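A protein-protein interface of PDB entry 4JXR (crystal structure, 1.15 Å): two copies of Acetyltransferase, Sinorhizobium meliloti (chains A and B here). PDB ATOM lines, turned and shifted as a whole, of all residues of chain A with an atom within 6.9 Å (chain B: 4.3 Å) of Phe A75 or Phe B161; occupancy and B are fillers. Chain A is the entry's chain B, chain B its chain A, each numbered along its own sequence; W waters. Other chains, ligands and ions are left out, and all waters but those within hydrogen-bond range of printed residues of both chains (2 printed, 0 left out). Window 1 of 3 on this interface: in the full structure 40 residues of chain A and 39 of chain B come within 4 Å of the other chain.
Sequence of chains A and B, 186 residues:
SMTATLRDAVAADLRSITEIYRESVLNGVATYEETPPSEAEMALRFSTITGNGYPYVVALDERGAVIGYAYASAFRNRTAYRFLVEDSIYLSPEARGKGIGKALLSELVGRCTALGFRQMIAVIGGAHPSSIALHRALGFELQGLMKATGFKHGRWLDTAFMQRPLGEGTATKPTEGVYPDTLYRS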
ATOM      1  N   TYR A  54       7.116  -1.858  -2.253  1.00  0.00           N
ATOM      2  CA  TYR A  54       6.429  -0.598  -2.124  1.00  0.00           C
ATOM      3  C   TYR A  54       4.937  -0.770  -1.980  1.00  0.00           C
ATOM      4  O   TYR A  54       4.345  -1.708  -2.570  1.00  0.00           O
ATOM      5  CB  TYR A  54       6.718   0.253  -3.363  1.00  0.00           C
ATOM      6  CG  TYR A  54       8.145   0.655  -3.597  1.00  0.00           C
ATOM      7  CD1 TYR A  54       8.855   1.428  -2.691  1.00  0.00           C
ATOM      8  CD2 TYR A  54       8.792   0.360  -4.771  1.00  0.00           C
ATOM      9  CE1 TYR A  54      10.111   1.849  -2.935  1.00  0.00           C
ATOM     10  CE2 TYR A  54      10.055   0.771  -5.037  1.00  0.00           C
ATOM     11  CZ  TYR A  54      10.756   1.558  -4.123  1.00  0.00           C
ATOM     12  OH  TYR A  54      12.003   1.965  -4.429  1.00  0.00           O
ATOM     13  N   SER A  73       6.942   4.513  -5.314  1.00  0.00           N
ATOM     14  CA  SER A  73       7.970   3.805  -6.053  1.00  0.00           C
ATOM     15  C   SER A  73       9.273   4.581  -5.994  1.00  0.00           C
ATOM     16  O   SER A  73       9.370   5.625  -5.350  1.00  0.00           O
ATOM     17  CB  SER A  73       7.501   3.551  -7.495  1.00  0.00           C
ATOM     18  OG  SER A  73       8.400   2.635  -8.118  1.00  0.00           O
ATOM     19  N   ALA A  74      10.310   4.089  -6.645  1.00  0.00           N
ATOM     20  CA  ALA A  74      11.569   4.821  -6.680  1.00  0.00           C
ATOM     21  C   ALA A  74      11.392   6.122  -7.430  1.00  0.00           C
ATOM     22  O   ALA A  74      10.689   6.175  -8.434  1.00  0.00           O
ATOM     23  CB  ALA A  74      12.644   4.001  -7.362  1.00  0.00           C
ATOM     24  N   PHE A  75      12.122   7.142  -7.027  1.00  0.00           N
ATOM     25  CA  PHE A  75      12.340   8.314  -7.866  1.00  0.00           C
ATOM     26  C   PHE A  75      13.219   7.950  -9.037  1.00  0.00           C
ATOM     27  O   PHE A  75      12.898   8.195 -10.176  1.00  0.00           O
ATOM     28  CB  PHE A  75      12.954   9.416  -6.999  1.00  0.00           C
ATOM     29  CG  PHE A  75      13.444  10.593  -7.784  1.00  0.00           C
ATOM     30  CD1 PHE A  75      12.575  11.402  -8.443  1.00  0.00           C
ATOM     31  CD2 PHE A  75      14.778  10.903  -7.856  1.00  0.00           C
ATOM     32  CE1 PHE A  75      13.013  12.486  -9.214  1.00  0.00           C
ATOM     33  CE2 PHE A  75      15.243  11.938  -8.613  1.00  0.00           C
ATOM     34  CZ  PHE A  75      14.366  12.723  -9.306  1.00  0.00           C
ATOM     35  N   ARG A  76      14.353   7.361  -8.743  1.00  0.00           N
ATOM     36  CA  ARG A  76      15.286   6.766  -9.667  1.00  0.00           C
ATOM     37  C   ARG A  76      15.803   5.498  -8.877  1.00  0.00           C
ATOM     38  O   ARG A  76      16.006   5.540  -7.683  1.00  0.00           O
ATOM     39  CB  ARG A  76      16.440   7.678 -10.028  1.00  0.00           C
ATOM     40  CG  ARG A  76      16.027   8.769 -10.951  1.00  0.00           C
ATOM     41  CD  ARG A  76      17.105   9.780 -11.339  1.00  0.00           C
ATOM     42  NE  ARG A  76      16.653  10.500 -12.506  1.00  0.00           N
ATOM     43  CZ  ARG A  76      17.331  11.443 -13.190  1.00  0.00           C
ATOM     44  NH1 ARG A  76      18.510  11.872 -12.803  1.00  0.00           N
ATOM     45  NH2 ARG A  76      16.811  11.918 -14.299  1.00  0.00           N
ATOM     46  N   ASN A  77      16.026   4.417  -9.583  1.00  0.00           N
ATOM     47  CA  ASN A  77      16.383   3.170  -8.909  1.00  0.00           C
ATOM     48  C   ASN A  77      17.883   2.995  -8.780  1.00  0.00           C
ATOM     49  O   ASN A  77      18.362   1.886  -8.658  1.00  0.00           O
ATOM     50  CB  ASN A  77      15.739   1.971  -9.588  1.00  0.00           C
ATOM     51  CG  ASN A  77      16.241   1.775 -10.982  1.00  0.00           C
ATOM     52  OD1 ASN A  77      17.016   2.557 -11.487  1.00  0.00           O
ATOM     53  ND2 ASN A  77      15.811   0.696 -11.609  1.00  0.00           N
ATOM     54  N   ARG A  78      18.627   4.093  -8.857  1.00  0.00           N
ATOM     55  CA  ARG A  78      20.033   4.000  -8.318  1.00  0.00           C
ATOM     56  C   ARG A  78      20.211   3.836  -6.733  1.00  0.00           C
ATOM     57  O   ARG A  78      19.386   4.251  -5.942  1.00  0.00           O
ATOM     58  CB  ARG A  78      20.860   5.191  -8.789  1.00  0.00           C
ATOM     59  CG  ARG A  78      20.832   5.426 -10.301  1.00  0.00           C
ATOM     60  CD  ARG A  78      21.805   4.515 -11.010  1.00  0.00           C
ATOM     61  NE  ARG A  78      21.952   4.826 -12.438  1.00  0.00           N
ATOM     62  CZ  ARG A  78      21.670   3.989 -13.435  1.00  0.00           C
ATOM     63  NH1 ARG A  78      21.209   2.772 -13.184  1.00  0.00           N
ATOM     64  NH2 ARG A  78      21.859   4.368 -14.689  1.00  0.00           N
ATOM     65  N   TYR A  81      19.636   6.333  -3.908  1.00  0.00           N
ATOM     66  CA  TYR A  81      18.291   6.865  -3.745  1.00  0.00           C
ATOM     67  C   TYR A  81      17.354   5.909  -2.979  1.00  0.00           C
ATOM     68  O   TYR A  81      16.161   6.175  -2.895  1.00  0.00           O
ATOM     69  CB  TYR A  81      17.650   7.173  -5.092  1.00  0.00           C
ATOM     70  CG  TYR A  81      18.146   8.379  -5.848  1.00  0.00           C
ATOM     71  CD1 TYR A  81      18.036   9.666  -5.318  1.00  0.00           C
ATOM     72  CD2 TYR A  81      18.633   8.262  -7.138  1.00  0.00           C
ATOM     73  CE1 TYR A  81      18.330  10.791  -6.072  1.00  0.00           C
ATOM     74  CE2 TYR A  81      18.966   9.389  -7.891  1.00  0.00           C
ATOM     75  CZ  TYR A  81      18.802  10.652  -7.349  1.00  0.00           C
ATOM     76  OH  TYR A  81      19.106  11.775  -8.111  1.00  0.00           O
ATOM     77  N   LEU A  84      14.603   7.106  -0.628  1.00  0.00           N
ATOM     78  CA  LEU A  84      13.690   8.095  -1.208  1.00  0.00           C
ATOM     79  C   LEU A  84      12.592   7.365  -1.995  1.00  0.00           C
ATOM     80  O   LEU A  84      12.914   6.478  -2.819  1.00  0.00           O
ATOM     81  CB  LEU A  84      14.483   8.987  -2.161  1.00  0.00           C
ATOM     82  CG  LEU A  84      13.690   9.936  -3.037  1.00  0.00           C
ATOM     83  CD1 LEU A  84      12.901  10.967  -2.219  1.00  0.00           C
ATOM     84  CD2 LEU A  84      14.605  10.608  -4.041  1.00  0.00           C
ATOM     85  N   VAL A  85      11.351   7.757  -1.796  1.00  0.00           N
ATOM     86  CA  VAL A  85      10.248   7.273  -2.591  1.00  0.00           C
ATOM     87  C   VAL A  85       9.541   8.442  -3.233  1.00  0.00           C
ATOM     88  O   VAL A  85       9.617   9.576  -2.761  1.00  0.00           O
ATOM     89  CB  VAL A  85       9.231   6.462  -1.758  1.00  0.00           C
ATOM     90  CG1 VAL A  85       9.743   5.055  -1.495  1.00  0.00           C
ATOM     91  CG2 VAL A  85       8.892   7.139  -0.406  1.00  0.00           C
ATOM     92  N   GLU A  86       8.801   8.144  -4.291  1.00  0.00           N
ATOM     93  CA  GLU A  86       7.986   9.091  -5.012  1.00  0.00           C
ATOM     94  C   GLU A  86       6.555   8.618  -4.986  1.00  0.00           C
ATOM     95  O   GLU A  86       6.293   7.432  -5.240  1.00  0.00           O
ATOM     96  CB  GLU A  86       8.498   9.193  -6.456  1.00  0.00           C
ATOM     97  CG  GLU A  86       7.653  10.091  -7.338  1.00  0.00           C
ATOM     98  CD  GLU A  86       8.196  10.323  -8.710  1.00  0.00           C
ATOM     99  OE1 GLU A  86       9.364   9.977  -8.964  1.00  0.00           O
ATOM    100  OE2 GLU A  86       7.472  10.856  -9.581  1.00  0.00           O
ATOM    101  N   ILE A 121       9.242  12.373  -2.419  1.00  0.00           N
ATOM    102  CA  ILE A 121       9.170  13.408  -3.433  1.00  0.00           C
ATOM    103  C   ILE A 121       7.902  13.217  -4.248  1.00  0.00           C
ATOM    104  O   ILE A 121       7.493  12.106  -4.579  1.00  0.00           O
ATOM    105  CB  ILE A 121      10.461  13.379  -4.322  1.00  0.00           C
ATOM    106  CG1 ILE A 121      10.577  14.534  -5.293  1.00  0.00           C
ATOM    107  CG2 ILE A 121      10.676  12.047  -5.062  1.00  0.00           C
ATOM    108  CD1 ILE A 121      12.000  14.620  -5.795  1.00  0.00           C
ATOM    109  N   VAL A 123       6.455  14.624  -7.913  1.00  0.00           N
ATOM    110  CA  VAL A 123       6.768  15.263  -9.177  1.00  0.00           C
ATOM    111  C   VAL A 123       5.427  15.567  -9.823  1.00  0.00           C
ATOM    112  O   VAL A 123       4.762  14.668 -10.295  1.00  0.00           O
ATOM    113  CB  VAL A 123       7.667  14.375 -10.057  1.00  0.00           C
ATOM    114  CG1 VAL A 123       7.991  15.082 -11.368  1.00  0.00           C
ATOM    115  CG2 VAL A 123       8.934  14.034  -9.300  1.00  0.00           C
ATOM    116  N   MET A 146      10.297  23.364 -12.410  1.00  0.00           N
ATOM    117  CA  MET A 146      11.101  23.145 -13.617  1.00  0.00           C
ATOM    118  C   MET A 146      10.230  23.590 -14.777  1.00  0.00           C
ATOM    119  O   MET A 146       9.311  22.900 -15.223  1.00  0.00           O
ATOM    120  CB  MET A 146      11.505  21.700 -13.759  1.00  0.00           C
ATOM    121  CG  MET A 146      12.076  21.080 -12.507  1.00  0.00           C
ATOM    122  SD  MET A 146      13.699  21.937 -11.881  1.00  0.00           S
ATOM    123  CE  MET A 146      13.413  21.376  -9.979  1.00  0.00           C
ATOM    124  N   PHE A 161       8.303  20.139  -8.110  1.00  0.00           N
ATOM    125  CA  PHE A 161       8.904  19.134  -7.252  1.00  0.00           C
ATOM    126  C   PHE A 161       8.676  19.510  -5.805  1.00  0.00           C
ATOM    127  O   PHE A 161       9.029  20.619  -5.391  1.00  0.00           O
ATOM    128  CB  PHE A 161      10.409  19.041  -7.497  1.00  0.00           C
ATOM    129  CG  PHE A 161      10.765  18.386  -8.816  1.00  0.00           C
ATOM    130  CD1 PHE A 161      10.402  18.963 -10.039  1.00  0.00           C
ATOM    131  CD2 PHE A 161      11.343  17.151  -8.871  1.00  0.00           C
ATOM    132  CE1 PHE A 161      10.671  18.307 -11.261  1.00  0.00           C
ATOM    133  CE2 PHE A 161      11.647  16.545 -10.092  1.00  0.00           C
ATOM    134  CZ  PHE A 161      11.300  17.155 -11.259  1.00  0.00           C
ATOM    135  N   TYR A 184      18.150  -2.287  -4.257  1.00  0.00           N
ATOM    136  CA  TYR A 184      19.052  -1.748  -5.294  1.00  0.00           C
ATOM    137  C   TYR A 184      20.528  -2.033  -4.942  1.00  0.00           C
ATOM    138  O   TYR A 184      21.401  -1.222  -5.234  1.00  0.00           O
ATOM    139  CB  TYR A 184      18.797  -0.250  -5.636  1.00  0.00           C
ATOM    140  CG  TYR A 184      17.317   0.032  -5.845  1.00  0.00           C
ATOM    141  CD1 TYR A 184      16.537  -0.811  -6.646  1.00  0.00           C
ATOM    142  CD2 TYR A 184      16.704   1.086  -5.210  1.00  0.00           C
ATOM    143  CE1 TYR A 184      15.193  -0.613  -6.777  1.00  0.00           C
ATOM    144  CE2 TYR A 184      15.326   1.324  -5.362  1.00  0.00           C
ATOM    145  CZ  TYR A 184      14.586   0.446  -6.157  1.00  0.00           C
ATOM    146  OH  TYR A 184      13.252   0.590  -6.306  1.00  0.00           O
ATOM    147  N   ARG B  76      13.364  11.857 -18.079  1.00  0.00           N
ATOM    148  CA  ARG B  76      12.482  10.717 -18.034  1.00  0.00           C
ATOM    149  C   ARG B  76      11.978  10.501 -19.458  1.00  0.00           C
ATOM    150  O   ARG B  76      11.736  11.442 -20.169  1.00  0.00           O
ATOM    151  CB  ARG B  76      11.281  10.921 -17.091  1.00  0.00           C
ATOM    152  CG  ARG B  76      11.657  10.978 -15.653  1.00  0.00           C
ATOM    153  CD  ARG B  76      10.547  11.191 -14.607  1.00  0.00           C
ATOM    154  NE  ARG B  76      11.064  10.842 -13.286  1.00  0.00           N
ATOM    155  CZ  ARG B  76      10.351  10.846 -12.154  1.00  0.00           C
ATOM    156  NH1 ARG B  76       9.120  11.323 -12.120  1.00  0.00           N
ATOM    157  NH2 ARG B  76      10.896  10.405 -11.053  1.00  0.00           N
ATOM    158  N   ILE B 121      18.281  20.034 -18.107  1.00  0.00           N
ATOM    159  CA  ILE B 121      18.356  19.902 -16.653  1.00  0.00           C
ATOM    160  C   ILE B 121      19.621  19.181 -16.274  1.00  0.00           C
ATOM    161  O   ILE B 121      20.066  18.261 -16.947  1.00  0.00           O
ATOM    162  CB  ILE B 121      17.051  19.186 -16.127  1.00  0.00           C
ATOM    163  CG1 ILE B 121      16.889  19.155 -14.613  1.00  0.00           C
ATOM    164  CG2 ILE B 121      16.931  17.772 -16.646  1.00  0.00           C
ATOM    165  CD1 ILE B 121      15.466  18.774 -14.184  1.00  0.00           C
ATOM    166  N   ALA B 122      20.217  19.612 -15.166  1.00  0.00           N
ATOM    167  CA  ALA B 122      21.301  18.916 -14.507  1.00  0.00           C
ATOM    168  C   ALA B 122      20.803  18.484 -13.120  1.00  0.00           C
ATOM    169  O   ALA B 122      20.230  19.269 -12.388  1.00  0.00           O
ATOM    170  CB  ALA B 122      22.521  19.789 -14.363  1.00  0.00           C
ATOM    171  N   VAL B 123      21.033  17.226 -12.816  1.00  0.00           N
ATOM    172  CA  VAL B 123      20.695  16.630 -11.517  1.00  0.00           C
ATOM    173  C   VAL B 123      22.014  16.302 -10.868  1.00  0.00           C
ATOM    174  O   VAL B 123      22.700  15.369 -11.309  1.00  0.00           O
ATOM    175  CB  VAL B 123      19.799  15.397 -11.680  1.00  0.00           C
ATOM    176  CG1 VAL B 123      19.503  14.821 -10.291  1.00  0.00           C
ATOM    177  CG2 VAL B 123      18.535  15.726 -12.434  1.00  0.00           C
ATOM    178  N   LEU B 142      20.117  27.453 -10.594  1.00  0.00           N
ATOM    179  CA  LEU B 142      19.668  26.554  -9.565  1.00  0.00           C
ATOM    180  C   LEU B 142      18.163  26.645  -9.394  1.00  0.00           C
ATOM    181  O   LEU B 142      17.621  27.724  -9.208  1.00  0.00           O
ATOM    182  CB  LEU B 142      20.425  26.878  -8.254  1.00  0.00           C
ATOM    183  CG  LEU B 142      20.179  25.950  -7.077  1.00  0.00           C
ATOM    184  CD1 LEU B 142      20.654  24.547  -7.339  1.00  0.00           C
ATOM    185  CD2 LEU B 142      20.866  26.519  -5.847  1.00  0.00           C
ATOM    186  N   GLN B 143      17.484  25.527  -9.491  1.00  0.00           N
ATOM    187  CA  GLN B 143      16.074  25.444  -9.337  1.00  0.00           C
ATOM    188  C   GLN B 143      15.634  24.889  -8.021  1.00  0.00           C
ATOM    189  O   GLN B 143      14.506  25.181  -7.579  1.00  0.00           O
ATOM    190  CB  GLN B 143      15.458  24.619 -10.446  1.00  0.00           C
ATOM    191  CG  GLN B 143      15.733  25.105 -11.836  1.00  0.00           C
ATOM    192  CD  GLN B 143      15.284  26.517 -12.029  1.00  0.00           C
ATOM    193  OE1 GLN B 143      14.127  26.858 -11.681  1.00  0.00           O
ATOM    194  NE2 GLN B 143      16.109  27.335 -12.622  1.00  0.00           N
ATOM    195  N   GLY B 144      16.424  24.068  -7.375  1.00  0.00           N
ATOM    196  CA  GLY B 144      16.072  23.537  -6.057  1.00  0.00           C
ATOM    197  C   GLY B 144      17.097  22.583  -5.588  1.00  0.00           C
ATOM    198  O   GLY B 144      18.004  22.157  -6.315  1.00  0.00           O
ATOM    199  N   MET B 146      17.139  19.104  -3.287  1.00  0.00           N
ATOM    200  CA  MET B 146      16.332  18.028  -2.685  1.00  0.00           C
ATOM    201  C   MET B 146      17.207  17.431  -1.600  1.00  0.00           C
ATOM    202  O   MET B 146      18.159  16.647  -1.849  1.00  0.00           O
ATOM    203  CB  MET B 146      15.907  16.935  -3.684  1.00  0.00           C
ATOM    204  CG  MET B 146      15.513  17.380  -5.078  1.00  0.00           C
ATOM    205  SD  MET B 146      14.021  18.647  -5.172  1.00  0.00           S
ATOM    206  CE  MET B 146      12.635  17.628  -4.192  1.00  0.00           C
ATOM    207  N   THR B 159      20.705  16.649  -3.388  1.00  0.00           N
ATOM    208  CA  THR B 159      20.721  16.538  -4.835  1.00  0.00           C
ATOM    209  C   THR B 159      20.231  17.863  -5.421  1.00  0.00           C
ATOM    210  O   THR B 159      19.118  18.260  -5.134  1.00  0.00           O
ATOM    211  CB  THR B 159      19.851  15.367  -5.312  1.00  0.00           C
ATOM    212  OG1 THR B 159      20.210  14.179  -4.581  1.00  0.00           O
ATOM    213  CG2 THR B 159      20.053  15.109  -6.779  1.00  0.00           C
ATOM    214  N   ALA B 160      21.072  18.550  -6.177  1.00  0.00           N
ATOM    215  CA  ALA B 160      20.711  19.862  -6.719  1.00  0.00           C
ATOM    216  C   ALA B 160      20.144  19.709  -8.115  1.00  0.00           C
ATOM    217  O   ALA B 160      20.591  18.883  -8.891  1.00  0.00           O
ATOM    218  CB  ALA B 160      21.901  20.781  -6.763  1.00  0.00           C
ATOM    219  N   PHE B 161      19.137  20.501  -8.429  1.00  0.00           N
ATOM    220  CA  PHE B 161      18.514  20.537  -9.764  1.00  0.00           C
ATOM    221  C   PHE B 161      18.777  21.898 -10.362  1.00  0.00           C
ATOM    222  O   PHE B 161      18.469  22.923  -9.735  1.00  0.00           O
ATOM    223  CB  PHE B 161      17.021  20.318  -9.660  1.00  0.00           C
ATOM    224  CG  PHE B 161      16.659  18.858  -9.379  1.00  0.00           C
ATOM    225  CD1 PHE B 161      17.041  18.195  -8.221  1.00  0.00           C
ATOM    226  CD2 PHE B 161      16.010  18.130 -10.292  1.00  0.00           C
ATOM    227  CE1 PHE B 161      16.714  16.860  -7.990  1.00  0.00           C
ATOM    228  CE2 PHE B 161      15.678  16.775 -10.055  1.00  0.00           C
ATOM    229  CZ  PHE B 161      16.072  16.192  -8.900  1.00  0.00           C
ATOM    230  N   MET B 162      19.329  21.919 -11.558  1.00  0.00           N
ATOM    231  CA  MET B 162      19.585  23.170 -12.277  1.00  0.00           C
ATOM    232  C   MET B 162      18.990  23.064 -13.660  1.00  0.00           C
ATOM    233  O   MET B 162      18.787  21.965 -14.181  1.00  0.00           O
ATOM    234  CB  MET B 162      21.061  23.451 -12.387  1.00  0.00           C
ATOM    235  CG  MET B 162      21.762  23.411 -11.012  1.00  0.00           C
ATOM    236  SD  MET B 162      23.607  23.952 -11.134  1.00  0.00           S
ATOM    237  CE  MET B 162      23.375  25.837 -11.383  1.00  0.00           C
HETATM  238  O   HOH W   1      12.966   8.132 -13.164  1.00  0.00           O
HETATM  239  O   HOH W   2      13.805  10.813 -12.953  1.00  0.00           O
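Arg A76 touches Val B123, and with the chains exchanged Val A123 touches Arg B76. Ile A121 touches Met B146, but with the chains exchanged Met A146 does not touch Ile B121 (4.3 Å). Met A146 touches Phe B161, but with the chains exchanged Phe A161 does not touch Met B146 (4.2 Å). Of the 10 pairs that touch across the chains among the printed residues, 2 have their exchanged pair printed and touching as well.
Of the 12 printed residues of chain B, 6 touch a printed residue of chain A. Hydrophobic or aromatic side chains of chain A that line the printed part of chain B: Phe A75, Tyr A81, Ile A121, Val A123 and Met A146. Among the printed residues, Asp or Glu carboxylates within 4 Å of a Lys or Arg side-chain nitrogen of the other chain: Glu A86 with Arg B76 (2.6 Å).
The guanidinium group of Arg B76 sits at hydrogen-bond distance from the backbone carbonyl oxygen of Phe A75. The guanidinium group (NH2) of Arg B76 is in salt-bridge range of the side-chain carboxylate (OE1) of Glu A86 (2.6 Å).
Of chain B, only Arg B76 (3.1 Å) and Phe B161 (3.9 Å) come within 4 Å of Phe A75. Of the printed residues of chain B, Met A146 touches Gln B143 (3.5 Å) and Phe B161 (3.8 Å). Tyr A184 touches none of the printed residues of chain B. Printed residues of chain A within 4 Å of Val B123: Arg A76 and Tyr A81. Of the printed residues of chain A, Phe B161 touches Phe A75 (3.9 Å) and Met A146 (3.8 Å).
O of Ser A73 lies within hydrogen-bond range of N of Glu A86 (2.8 Å). O of Phe B161 is in hydrogen-bond range of N of Gln B143, 2.8 Å away. The backbone carbonyl oxygen of Thr B159 sits at hydrogen-bond distance from the backbone NH of Met B146 (2.8 Å). The backbone NH of Phe B161 lies within hydrogen-bond range of the backbone carbonyl oxygen of Gly B144. The backbone carbonyl oxygen of Val A85 lies within hydrogen-bond range of the backbone NH of Ile A121 (2.8 Å).
Water W2 bridges NE of Arg B76 and NE of Arg A76. Water W1 lies within hydrogen-bond range of O of Phe A75 (3.0 Å) and NE of Arg B76 (3.3 Å).
Among the printed residues, merely in contact across the chains: Phe A75 with Phe B161 (3.9 Å), Arg A76 with Val B123 (3.9 Å), Tyr A81 with Val B123 (3.8 Å), Tyr A81 with Thr B159 (3.7 Å), Ile A121 with Met B146 (3.5 Å), Val A123 with Arg B76 (3.9 Å), Met A146 with Gln B143 (3.5 Å) and Met A146 with Phe B161 (3.8 Å).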
